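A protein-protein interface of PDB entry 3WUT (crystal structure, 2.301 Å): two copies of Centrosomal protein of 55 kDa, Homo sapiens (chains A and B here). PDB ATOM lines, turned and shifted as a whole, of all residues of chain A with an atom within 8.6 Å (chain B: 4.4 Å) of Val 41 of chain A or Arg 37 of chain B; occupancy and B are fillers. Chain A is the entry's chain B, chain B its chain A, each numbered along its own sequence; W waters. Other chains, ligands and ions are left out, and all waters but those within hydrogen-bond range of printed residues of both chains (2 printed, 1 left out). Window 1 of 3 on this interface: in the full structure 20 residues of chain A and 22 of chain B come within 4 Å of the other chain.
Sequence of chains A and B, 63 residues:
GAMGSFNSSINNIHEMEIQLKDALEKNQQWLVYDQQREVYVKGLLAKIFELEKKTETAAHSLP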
ATOM      1  N   TRP A  30      28.879  -8.440 -27.315  1.00  0.00           N
ATOM      2  CA  TRP A  30      29.478  -8.498 -25.988  1.00  0.00           C
ATOM      3  C   TRP A  30      28.970  -7.326 -25.178  1.00  0.00           C
ATOM      4  O   TRP A  30      28.628  -7.465 -24.010  1.00  0.00           O
ATOM      5  CB  TRP A  30      31.004  -8.410 -26.069  1.00  0.00           C
ATOM      6  CG  TRP A  30      31.663  -9.693 -26.425  1.00  0.00           C
ATOM      7  CD1 TRP A  30      32.127 -10.059 -27.651  1.00  0.00           C
ATOM      8  CD2 TRP A  30      31.935 -10.794 -25.546  1.00  0.00           C
ATOM      9  NE1 TRP A  30      32.671 -11.323 -27.595  1.00  0.00           N
ATOM     10  CE2 TRP A  30      32.565 -11.796 -26.312  1.00  0.00           C
ATOM     11  CE3 TRP A  30      31.704 -11.033 -24.186  1.00  0.00           C
ATOM     12  CZ2 TRP A  30      32.974 -13.011 -25.767  1.00  0.00           C
ATOM     13  CZ3 TRP A  30      32.107 -12.243 -23.646  1.00  0.00           C
ATOM     14  CH2 TRP A  30      32.734 -13.215 -24.435  1.00  0.00           C
ATOM     15  N   LEU A  31      28.939  -6.165 -25.816  1.00  0.00           N
ATOM     16  CA  LEU A  31      28.598  -4.924 -25.145  1.00  0.00           C
ATOM     17  C   LEU A  31      27.214  -4.958 -24.509  1.00  0.00           C
ATOM     18  O   LEU A  31      27.044  -4.524 -23.368  1.00  0.00           O
ATOM     19  CB  LEU A  31      28.674  -3.771 -26.134  1.00  0.00           C
ATOM     20  CG  LEU A  31      30.022  -3.077 -26.350  1.00  0.00           C
ATOM     21  CD1 LEU A  31      31.256  -3.932 -25.953  1.00  0.00           C
ATOM     22  CD2 LEU A  31      30.103  -2.592 -27.804  1.00  0.00           C
ATOM     23  N   VAL A  32      26.238  -5.466 -25.254  1.00  0.00           N
ATOM     24  CA  VAL A  32      24.864  -5.506 -24.785  1.00  0.00           C
ATOM     25  C   VAL A  32      24.718  -6.612 -23.757  1.00  0.00           C
ATOM     26  O   VAL A  32      24.034  -6.449 -22.748  1.00  0.00           O
ATOM     27  CB  VAL A  32      23.884  -5.755 -25.936  1.00  0.00           C
ATOM     28  CG1 VAL A  32      22.467  -5.804 -25.410  1.00  0.00           C
ATOM     29  CG2 VAL A  32      24.029  -4.667 -26.984  1.00  0.00           C
ATOM     30  N   TYR A  33      25.375  -7.736 -24.026  1.00  0.00           N
ATOM     31  CA  TYR A  33      25.435  -8.855 -23.099  1.00  0.00           C
ATOM     32  C   TYR A  33      26.029  -8.408 -21.769  1.00  0.00           C
ATOM     33  O   TYR A  33      25.527  -8.774 -20.716  1.00  0.00           O
ATOM     34  CB  TYR A  33      26.264  -9.978 -23.718  1.00  0.00           C
ATOM     35  CG  TYR A  33      26.736 -11.074 -22.780  1.00  0.00           C
ATOM     36  CD1 TYR A  33      25.911 -12.132 -22.442  1.00  0.00           C
ATOM     37  CD2 TYR A  33      28.025 -11.070 -22.266  1.00  0.00           C
ATOM     38  CE1 TYR A  33      26.350 -13.153 -21.599  1.00  0.00           C
ATOM     39  CE2 TYR A  33      28.471 -12.090 -21.426  1.00  0.00           C
ATOM     40  CZ  TYR A  33      27.634 -13.122 -21.092  1.00  0.00           C
ATOM     41  OH  TYR A  33      28.087 -14.125 -20.259  1.00  0.00           O
ATOM     42  N   ASP A  34      27.082  -7.596 -21.844  1.00  0.00           N
ATOM     43  CA  ASP A  34      27.770  -7.065 -20.678  1.00  0.00           C
ATOM     44  C   ASP A  34      26.856  -6.183 -19.830  1.00  0.00           C
ATOM     45  O   ASP A  34      26.919  -6.225 -18.600  1.00  0.00           O
ATOM     46  CB  ASP A  34      29.000  -6.265 -21.115  1.00  0.00           C
ATOM     47  CG  ASP A  34      29.741  -5.659 -19.950  1.00  0.00           C
ATOM     48  OD1 ASP A  34      30.466  -6.404 -19.263  1.00  0.00           O
ATOM     49  OD2 ASP A  34      29.602  -4.440 -19.711  1.00  0.00           O
ATOM     50  N   GLN A  35      26.029  -5.375 -20.491  1.00  0.00           N
ATOM     51  CA  GLN A  35      25.072  -4.516 -19.801  1.00  0.00           C
ATOM     52  C   GLN A  35      24.071  -5.348 -19.013  1.00  0.00           C
ATOM     53  O   GLN A  35      23.750  -5.022 -17.871  1.00  0.00           O
ATOM     54  CB  GLN A  35      24.307  -3.658 -20.797  1.00  0.00           C
ATOM     55  CG  GLN A  35      25.114  -2.539 -21.403  1.00  0.00           C
ATOM     56  CD  GLN A  35      24.297  -1.710 -22.376  1.00  0.00           C
ATOM     57  OE1 GLN A  35      23.569  -2.247 -23.214  1.00  0.00           O
ATOM     58  NE2 GLN A  35      24.411  -0.394 -22.267  1.00  0.00           N
ATOM     59  N   GLN A  36      23.571  -6.404 -19.646  1.00  0.00           N
ATOM     60  CA  GLN A  36      22.666  -7.330 -18.987  1.00  0.00           C
ATOM     61  C   GLN A  36      23.344  -7.988 -17.792  1.00  0.00           C
ATOM     62  O   GLN A  36      22.758  -8.048 -16.718  1.00  0.00           O
ATOM     63  CB  GLN A  36      22.141  -8.393 -19.956  1.00  0.00           C
ATOM     64  CG  GLN A  36      21.071  -9.293 -19.329  1.00  0.00           C
ATOM     65  CD  GLN A  36      20.574 -10.380 -20.263  1.00  0.00           C
ATOM     66  OE1 GLN A  36      20.870 -11.563 -20.072  1.00  0.00           O
ATOM     67  NE2 GLN A  36      19.793  -9.990 -21.263  1.00  0.00           N
ATOM     68  N   ARG A  37      24.581  -8.452 -17.962  1.00  0.00           N
ATOM     69  CA  ARG A  37      25.286  -9.131 -16.869  1.00  0.00           C
ATOM     70  C   ARG A  37      25.560  -8.213 -15.672  1.00  0.00           C
ATOM     71  O   ARG A  37      25.433  -8.637 -14.518  1.00  0.00           O
ATOM     72  CB  ARG A  37      26.581  -9.768 -17.368  1.00  0.00           C
ATOM     73  CG  ARG A  37      26.371 -10.823 -18.444  1.00  0.00           C
ATOM     74  CD  ARG A  37      25.466 -11.941 -17.955  1.00  0.00           C
ATOM     75  NE  ARG A  37      26.137 -12.789 -16.974  1.00  0.00           N
ATOM     76  CZ  ARG A  37      25.510 -13.578 -16.108  1.00  0.00           C
ATOM     77  NH1 ARG A  37      24.178 -13.635 -16.084  1.00  0.00           N
ATOM     78  NH2 ARG A  37      26.218 -14.312 -15.254  1.00  0.00           N
ATOM     79  N   GLU A  38      25.905  -6.956 -15.946  1.00  0.00           N
ATOM     80  CA  GLU A  38      26.172  -5.991 -14.885  1.00  0.00           C
ATOM     81  C   GLU A  38      24.915  -5.690 -14.066  1.00  0.00           C
ATOM     82  O   GLU A  38      24.992  -5.552 -12.847  1.00  0.00           O
ATOM     83  CB  GLU A  38      26.774  -4.697 -15.456  1.00  0.00           C
ATOM     84  CG  GLU A  38      28.283  -4.758 -15.722  1.00  0.00           C
ATOM     85  CD  GLU A  38      29.061  -5.184 -14.492  1.00  0.00           C
ATOM     86  OE1 GLU A  38      29.445  -6.370 -14.401  1.00  0.00           O
ATOM     87  OE2 GLU A  38      29.292  -4.330 -13.614  1.00  0.00           O
ATOM     88  N   VAL A  39      23.764  -5.592 -14.736  1.00  0.00           N
ATOM     89  CA  VAL A  39      22.479  -5.460 -14.045  1.00  0.00           C
ATOM     90  C   VAL A  39      22.259  -6.669 -13.138  1.00  0.00           C
ATOM     91  O   VAL A  39      21.795  -6.531 -12.008  1.00  0.00           O
ATOM     92  CB  VAL A  39      21.310  -5.359 -15.051  1.00  0.00           C
ATOM     93  CG1 VAL A  39      19.939  -5.569 -14.359  1.00  0.00           C
ATOM     94  CG2 VAL A  39      21.368  -4.026 -15.806  1.00  0.00           C
ATOM     95  N   TYR A  40      22.613  -7.850 -13.641  1.00  0.00           N
ATOM     96  CA  TYR A  40      22.475  -9.094 -12.890  1.00  0.00           C
ATOM     97  C   TYR A  40      23.394  -9.149 -11.661  1.00  0.00           C
ATOM     98  O   TYR A  40      22.961  -9.551 -10.578  1.00  0.00           O
ATOM     99  CB  TYR A  40      22.723 -10.293 -13.802  1.00  0.00           C
ATOM    100  CG  TYR A  40      22.766 -11.613 -13.066  1.00  0.00           C
ATOM    101  CD1 TYR A  40      21.601 -12.240 -12.653  1.00  0.00           C
ATOM    102  CD2 TYR A  40      23.974 -12.232 -12.782  1.00  0.00           C
ATOM    103  CE1 TYR A  40      21.639 -13.453 -11.971  1.00  0.00           C
ATOM    104  CE2 TYR A  40      24.021 -13.443 -12.094  1.00  0.00           C
ATOM    105  CZ  TYR A  40      22.856 -14.050 -11.691  1.00  0.00           C
ATOM    106  OH  TYR A  40      22.924 -15.258 -11.016  1.00  0.00           O
ATOM    107  N   VAL A  41      24.652  -8.739 -11.830  1.00  0.00           N
ATOM    108  CA  VAL A  41      25.593  -8.692 -10.720  1.00  0.00           C
ATOM    109  C   VAL A  41      25.102  -7.722  -9.649  1.00  0.00           C
ATOM    110  O   VAL A  41      25.156  -8.031  -8.462  1.00  0.00           O
ATOM    111  CB  VAL A  41      27.000  -8.237 -11.161  1.00  0.00           C
ATOM    112  CG1 VAL A  41      27.898  -8.044  -9.936  1.00  0.00           C
ATOM    113  CG2 VAL A  41      27.620  -9.232 -12.143  1.00  0.00           C
ATOM    114  N   LYS A  42      24.620  -6.551 -10.068  1.00  0.00           N
ATOM    115  CA  LYS A  42      24.101  -5.570  -9.115  1.00  0.00           C
ATOM    116  C   LYS A  42      22.874  -6.073  -8.361  1.00  0.00           C
ATOM    117  O   LYS A  42      22.692  -5.758  -7.184  1.00  0.00           O
ATOM    118  CB  LYS A  42      23.793  -4.249  -9.811  1.00  0.00           C
ATOM    119  CG  LYS A  42      25.043  -3.558 -10.312  1.00  0.00           C
ATOM    120  CD  LYS A  42      24.718  -2.269 -11.038  1.00  0.00           C
ATOM    121  CE  LYS A  42      26.001  -1.607 -11.490  1.00  0.00           C
ATOM    122  NZ  LYS A  42      25.769  -0.678 -12.629  1.00  0.00           N
ATOM    123  N   GLY A  43      22.046  -6.859  -9.040  1.00  0.00           N
ATOM    124  CA  GLY A  43      20.892  -7.478  -8.420  1.00  0.00           C
ATOM    125  C   GLY A  43      21.281  -8.442  -7.325  1.00  0.00           C
ATOM    126  O   GLY A  43      20.632  -8.475  -6.280  1.00  0.00           O
ATOM    127  N   LEU A  44      22.329  -9.235  -7.551  1.00  0.00           N
ATOM    128  CA  LEU A  44      22.789 -10.181  -6.535  1.00  0.00           C
ATOM    129  C   LEU A  44      23.356  -9.454  -5.326  1.00  0.00           C
ATOM    130  O   LEU A  44      23.098  -9.841  -4.189  1.00  0.00           O
ATOM    131  CB  LEU A  44      23.841 -11.129  -7.093  1.00  0.00           C
ATOM    132  CG  LEU A  44      23.413 -12.064  -8.224  1.00  0.00           C
ATOM    133  CD1 LEU A  44      24.596 -12.960  -8.624  1.00  0.00           C
ATOM    134  CD2 LEU A  44      22.207 -12.877  -7.780  1.00  0.00           C
ATOM    135  N   LEU A  45      24.120  -8.397  -5.582  1.00  0.00           N
ATOM    136  CA  LEU A  45      24.679  -7.570  -4.523  1.00  0.00           C
ATOM    137  C   LEU A  45      23.603  -6.865  -3.701  1.00  0.00           C
ATOM    138  O   LEU A  45      23.750  -6.731  -2.485  1.00  0.00           O
ATOM    139  CB  LEU A  45      25.657  -6.549  -5.109  1.00  0.00           C
ATOM    140  CG  LEU A  45      26.980  -7.175  -5.577  1.00  0.00           C
ATOM    141  CD1 LEU A  45      27.817  -6.197  -6.406  1.00  0.00           C
ATOM    142  CD2 LEU A  45      27.754  -7.657  -4.368  1.00  0.00           C
ATOM    143  N   ALA A  46      22.532  -6.411  -4.362  1.00  0.00           N
ATOM    144  CA  ALA A  46      21.397  -5.792  -3.665  1.00  0.00           C
ATOM    145  C   ALA A  46      20.700  -6.812  -2.765  1.00  0.00           C
ATOM    146  O   ALA A  46      20.333  -6.506  -1.637  1.00  0.00           O
ATOM    147  CB  ALA A  46      20.397  -5.190  -4.667  1.00  0.00           C
ATOM    148  N   LYS A  47      20.537  -8.028  -3.273  1.00  0.00           N
ATOM    149  CA  LYS A  47      19.958  -9.111  -2.500  1.00  0.00           C
ATOM    150  C   LYS A  47      20.815  -9.447  -1.281  1.00  0.00           C
ATOM    151  O   LYS A  47      20.282  -9.650  -0.189  1.00  0.00           O
ATOM    152  CB  LYS A  47      19.776 -10.344  -3.376  1.00  0.00           C
ATOM    153  CG  LYS A  47      19.068 -11.498  -2.685  1.00  0.00           C
ATOM    154  CD  LYS A  47      18.672 -12.552  -3.702  1.00  0.00           C
ATOM    155  CE  LYS A  47      18.001 -13.741  -3.046  1.00  0.00           C
ATOM    156  NZ  LYS A  47      17.584 -14.742  -4.067  1.00  0.00           N
ATOM    157  N   ILE A  48      22.135  -9.503  -1.463  1.00  0.00           N
ATOM    158  CA  ILE A  48      23.048  -9.771  -0.356  1.00  0.00           C
ATOM    159  C   ILE A  48      22.937  -8.678   0.702  1.00  0.00           C
ATOM    160  O   ILE A  48      22.867  -8.956   1.901  1.00  0.00           O
ATOM    161  CB  ILE A  48      24.506  -9.853  -0.846  1.00  0.00           C
ATOM    162  CG1 ILE A  48      24.707 -11.104  -1.705  1.00  0.00           C
ATOM    163  CG2 ILE A  48      25.479  -9.824   0.331  1.00  0.00           C
ATOM    164  CD1 ILE A  48      26.068 -11.219  -2.352  1.00  0.00           C
ATOM    165  N   TYR B  33      37.617 -11.345 -19.310  1.00  0.00           N
ATOM    166  CA  TYR B  33      36.820 -10.502 -18.422  1.00  0.00           C
ATOM    167  C   TYR B  33      35.554 -11.209 -17.937  1.00  0.00           C
ATOM    168  O   TYR B  33      35.249 -11.199 -16.743  1.00  0.00           O
ATOM    169  CB  TYR B  33      36.419  -9.244 -19.183  1.00  0.00           C
ATOM    170  CG  TYR B  33      35.639  -8.215 -18.399  1.00  0.00           C
ATOM    171  CD1 TYR B  33      36.283  -7.337 -17.558  1.00  0.00           C
ATOM    172  CD2 TYR B  33      34.264  -8.086 -18.544  1.00  0.00           C
ATOM    173  CE1 TYR B  33      35.595  -6.378 -16.856  1.00  0.00           C
ATOM    174  CE2 TYR B  33      33.560  -7.116 -17.839  1.00  0.00           C
ATOM    175  CZ  TYR B  33      34.236  -6.269 -16.997  1.00  0.00           C
ATOM    176  OH  TYR B  33      33.579  -5.300 -16.286  1.00  0.00           O
ATOM    177  N   ASP B  34      34.821 -11.810 -18.874  1.00  0.00           N
ATOM    178  CA  ASP B  34      33.537 -12.424 -18.565  1.00  0.00           C
ATOM    179  C   ASP B  34      33.694 -13.714 -17.784  1.00  0.00           C
ATOM    180  O   ASP B  34      32.841 -14.051 -16.959  1.00  0.00           O
ATOM    181  CB  ASP B  34      32.713 -12.688 -19.824  1.00  0.00           C
ATOM    182  CG  ASP B  34      31.260 -13.029 -19.489  1.00  0.00           C
ATOM    183  OD1 ASP B  34      30.595 -12.171 -18.866  1.00  0.00           O
ATOM    184  OD2 ASP B  34      30.790 -14.147 -19.816  1.00  0.00           O
ATOM    185  N   GLN B  35      34.776 -14.439 -18.053  1.00  0.00           N
ATOM    186  CA  GLN B  35      35.083 -15.660 -17.321  1.00  0.00           C
ATOM    187  C   GLN B  35      35.297 -15.337 -15.847  1.00  0.00           C
ATOM    188  O   GLN B  35      34.844 -16.073 -14.971  1.00  0.00           O
ATOM    189  CB  GLN B  35      36.317 -16.352 -17.907  1.00  0.00           C
ATOM    190  CG  GLN B  35      36.029 -17.105 -19.193  1.00  0.00           C
ATOM    191  CD  GLN B  35      37.243 -17.834 -19.739  1.00  0.00           C
ATOM    192  OE1 GLN B  35      37.139 -18.969 -20.201  1.00  0.00           O
ATOM    193  NE2 GLN B  35      38.392 -17.178 -19.708  1.00  0.00           N
ATOM    194  N   GLN B  36      35.966 -14.221 -15.579  1.00  0.00           N
ATOM    195  CA  GLN B  36      36.179 -13.791 -14.209  1.00  0.00           C
ATOM    196  C   GLN B  36      34.881 -13.327 -13.542  1.00  0.00           C
ATOM    197  O   GLN B  36      34.700 -13.497 -12.329  1.00  0.00           O
ATOM    198  CB  GLN B  36      37.216 -12.681 -14.176  1.00  0.00           C
ATOM    199  CG  GLN B  36      38.600 -13.151 -14.576  1.00  0.00           C
ATOM    200  CD  GLN B  36      39.651 -12.090 -14.336  1.00  0.00           C
ATOM    201  OE1 GLN B  36      39.469 -11.196 -13.510  1.00  0.00           O
ATOM    202  NE2 GLN B  36      40.757 -12.183 -15.058  1.00  0.00           N
ATOM    203  N   ARG B  37      33.975 -12.743 -14.325  1.00  0.00           N
ATOM    204  CA  ARG B  37      32.688 -12.343 -13.779  1.00  0.00           C
ATOM    205  C   ARG B  37      31.887 -13.565 -13.349  1.00  0.00           C
ATOM    206  O   ARG B  37      31.245 -13.549 -12.303  1.00  0.00           O
ATOM    207  CB  ARG B  37      31.902 -11.504 -14.783  1.00  0.00           C
ATOM    208  CG  ARG B  37      30.461 -11.255 -14.372  1.00  0.00           C
ATOM    209  CD  ARG B  37      29.882 -10.002 -15.029  1.00  0.00           C
ATOM    210  NE  ARG B  37      30.011 -10.085 -16.475  1.00  0.00           N
ATOM    211  CZ  ARG B  37      30.070  -9.032 -17.284  1.00  0.00           C
ATOM    212  NH1 ARG B  37      29.994  -7.798 -16.799  1.00  0.00           N
ATOM    213  NH2 ARG B  37      30.209  -9.219 -18.588  1.00  0.00           N
ATOM    214  N   GLU B  38      31.946 -14.625 -14.143  1.00  0.00           N
ATOM    215  CA  GLU B  38      31.266 -15.863 -13.800  1.00  0.00           C
ATOM    216  C   GLU B  38      31.757 -16.398 -12.465  1.00  0.00           C
ATOM    217  O   GLU B  38      30.955 -16.829 -11.631  1.00  0.00           O
ATOM    218  CB  GLU B  38      31.446 -16.909 -14.896  1.00  0.00           C
ATOM    219  CG  GLU B  38      30.586 -16.665 -16.140  1.00  0.00           C
ATOM    220  CD  GLU B  38      29.114 -16.432 -15.812  1.00  0.00           C
ATOM    221  OE1 GLU B  38      28.505 -17.272 -15.106  1.00  0.00           O
ATOM    222  OE2 GLU B  38      28.560 -15.415 -16.277  1.00  0.00           O
ATOM    223  N   VAL B  39      33.073 -16.341 -12.253  1.00  0.00           N
ATOM    224  CA  VAL B  39      33.652 -16.783 -10.989  1.00  0.00           C
ATOM    225  C   VAL B  39      33.097 -15.947  -9.846  1.00  0.00           C
ATOM    226  O   VAL B  39      32.689 -16.475  -8.809  1.00  0.00           O
ATOM    227  CB  VAL B  39      35.168 -16.668 -11.040  1.00  0.00           C
ATOM    228  CG1 VAL B  39      35.783 -16.755  -9.647  1.00  0.00           C
ATOM    229  CG2 VAL B  39      35.738 -17.719 -12.017  1.00  0.00           C
ATOM    230  N   TYR B  40      33.052 -14.637 -10.048  1.00  0.00           N
ATOM    231  CA  TYR B  40      32.591 -13.742  -9.004  1.00  0.00           C
ATOM    232  C   TYR B  40      31.121 -14.011  -8.716  1.00  0.00           C
ATOM    233  O   TYR B  40      30.672 -14.019  -7.568  1.00  0.00           O
ATOM    234  CB  TYR B  40      32.776 -12.294  -9.447  1.00  0.00           C
ATOM    235  CG  TYR B  40      32.343 -11.305  -8.395  1.00  0.00           C
ATOM    236  CD1 TYR B  40      33.041 -11.181  -7.203  1.00  0.00           C
ATOM    237  CD2 TYR B  40      31.222 -10.514  -8.577  1.00  0.00           C
ATOM    238  CE1 TYR B  40      32.628 -10.273  -6.208  1.00  0.00           C
ATOM    239  CE2 TYR B  40      30.818  -9.602  -7.595  1.00  0.00           C
ATOM    240  CZ  TYR B  40      31.518  -9.491  -6.414  1.00  0.00           C
ATOM    241  OH  TYR B  40      31.102  -8.593  -5.451  1.00  0.00           O
ATOM    242  N   VAL B  41      30.379 -14.247  -9.782  1.00  0.00           N
ATOM    243  CA  VAL B  41      28.938 -14.414  -9.710  1.00  0.00           C
ATOM    244  C   VAL B  41      28.511 -15.742  -9.028  1.00  0.00           C
ATOM    245  O   VAL B  41      27.564 -15.758  -8.232  1.00  0.00           O
ATOM    246  CB  VAL B  41      28.365 -14.204 -11.127  1.00  0.00           C
ATOM    247  CG1 VAL B  41      27.588 -15.379 -11.614  1.00  0.00           C
ATOM    248  CG2 VAL B  41      27.596 -12.872 -11.214  1.00  0.00           C
ATOM    249  N   LEU B  44      29.033 -15.110  -5.320  1.00  0.00           N
ATOM    250  CA  LEU B  44      27.878 -14.403  -4.784  1.00  0.00           C
ATOM    251  C   LEU B  44      26.661 -15.300  -4.560  1.00  0.00           C
ATOM    252  O   LEU B  44      25.967 -15.137  -3.563  1.00  0.00           O
ATOM    253  CB  LEU B  44      27.491 -13.248  -5.697  1.00  0.00           C
ATOM    254  CG  LEU B  44      28.494 -12.109  -5.892  1.00  0.00           C
ATOM    255  CD1 LEU B  44      27.793 -10.937  -6.574  1.00  0.00           C
ATOM    256  CD2 LEU B  44      29.144 -11.694  -4.577  1.00  0.00           C
HETATM  257  O   HOH W   1      27.290 -16.077 -18.813  1.00  0.00           O
HETATM  258  O   HOH W   2      31.278  -4.122 -17.083  1.00  0.00           O
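OD2 of Asp 34 of chain B lies within hydrogen-bond range of OH of Tyr 33 of chain A.
The guanidinium group (NH1) of Arg 37 of chain B lies within salt-bridge range of the side-chain carboxylate (OD1) of Asp 34 of chain A, 2.9 Å away.
The guanidinium group (NH1) of Arg 37 of chain B lies within salt-bridge range of the side-chain carboxylate (OE1) of Glu 38 of chain A (2.8 Å).
The side-chain carboxylate (OE2) of Glu 38 of chain B is in salt-bridge range of the guanidinium group (NH2) of Arg 37 of chain A.
Water W1 bridges the side-chain hydroxyl (OH) of Tyr 33 of chain A and the side-chain carboxylate (OE2) of Glu 38 of chain B.
Water W2 lies within hydrogen-bond range of OH of Tyr 33 of chain B (2.7 Å) and OD2 of Asp 34 of chain A (3.1 Å).
OD1 of Asp 34 of chain B lies within salt-bridge range of NH2 of Arg 37 of chain B, at 3.0 Å.
Tyr 33 of chain A touches Asp 34 of chain B, and with the chains exchanged Asp 34 of chain A touches Tyr 33 of chain B.
Asp 34 of chain A touches Arg 37 of chain B, but with the chains exchanged Arg 37 of chain A does not touch Asp 34 of chain B (4.5 Å).
Arg 37 of chain A touches Glu 38 of chain B, and with the chains exchanged Glu 38 of chain A touches Arg 37 of chain B.
Val 41 of chain A touches Arg 37 of chain B, but with the chains exchanged Arg 37 of chain A does not touch Val 41 of chain B (4.03 Å).
Of the 15 pairs that touch across the chains among the printed residues, 7 have their exchanged pair printed and touching as well.
Val 41 of chain A touches just these residues of chain B: Arg 37 (3.7 Å) and Val 41 (3.8 Å).
Of chain A, only Asp 34, Arg 37, Glu 38 and Val 41 come within 4 Å of Arg 37 of chain B.
Printed residues of chain B within 4 Å of Tyr 33 of chain A: Asp 34 (2.7 Å).
Printed residues of chain A within 4 Å of Asp 34 of chain B: Trp 30 and Tyr 33.
Printed residues of chain A within 4 Å of Val 41 of chain B: Tyr 40 (3.7 Å), Val 41 (3.8 Å) and Leu 44 (3.96 Å).
Of the printed residues of chain A, Glu 38 of chain B touches Arg 37.
Of the printed residues of chain A, Tyr 33 of chain B touches Asp 34 (3.5 Å).
Val 39 of chain A touches none of the printed residues of chain B.
Gln 35 of chain B touches none of the printed residues of chain A.
The nearest residue of chain B that does not touch Val 41 of chain A is Tyr 40 of chain B (4.1 Å).
The nearest residue of chain A that does not touch Arg 37 of chain B is Tyr 33 of chain A (4.4 Å).
The nearest printed residue of chain A that does not touch Asp 34 of chain B is Arg 37 of chain A (4.5 Å).
Tyr 33 of chain B touches Asp 34 of chain A (CE2 to OD1, 3.5 Å).
CB of Arg 37 of chain A touches NE of Arg 37 of chain B, 3.6 Å away.
Val 41 of chain B touches Tyr 40 of chain A (CG2 to CE2, 3.7 Å).
CD of Arg 37 of chain B touches CG2 of Val 41 of chain A, at 3.7 Å.
Val 41 of chain A touches Val 41 of chain B (CG2 to CG2, 3.8 Å).
Leu 44 of chain A touches Val 41 of chain B.
Leu 44 of chain A touches Leu 44 of chain B (CB to CD1, 3.99 Å).
Leu 45 of chain A touches Tyr 40 of chain B (CD2 to OH, 3.6 Å).
CD2 of Leu 45 of chain A touches CD1 of Leu 44 of chain B, at 3.95 Å.
CD2 of Leu 44 of chain B touches CD1 of Ile 48 of chain A, at 3.8 Å.
Of the 10 printed residues of chain B, 7 touch a printed residue of chain A.
Hydrophobic or aromatic side chains of chain B within 4 Å of the printed part of chain A: Tyr 33, Tyr 40, Val 41 and Leu 44.
Of the 19 printed residues of chain A, 10 touch a printed residue of chain B.
Among the printed residues, 15 pairs touch across the chains.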
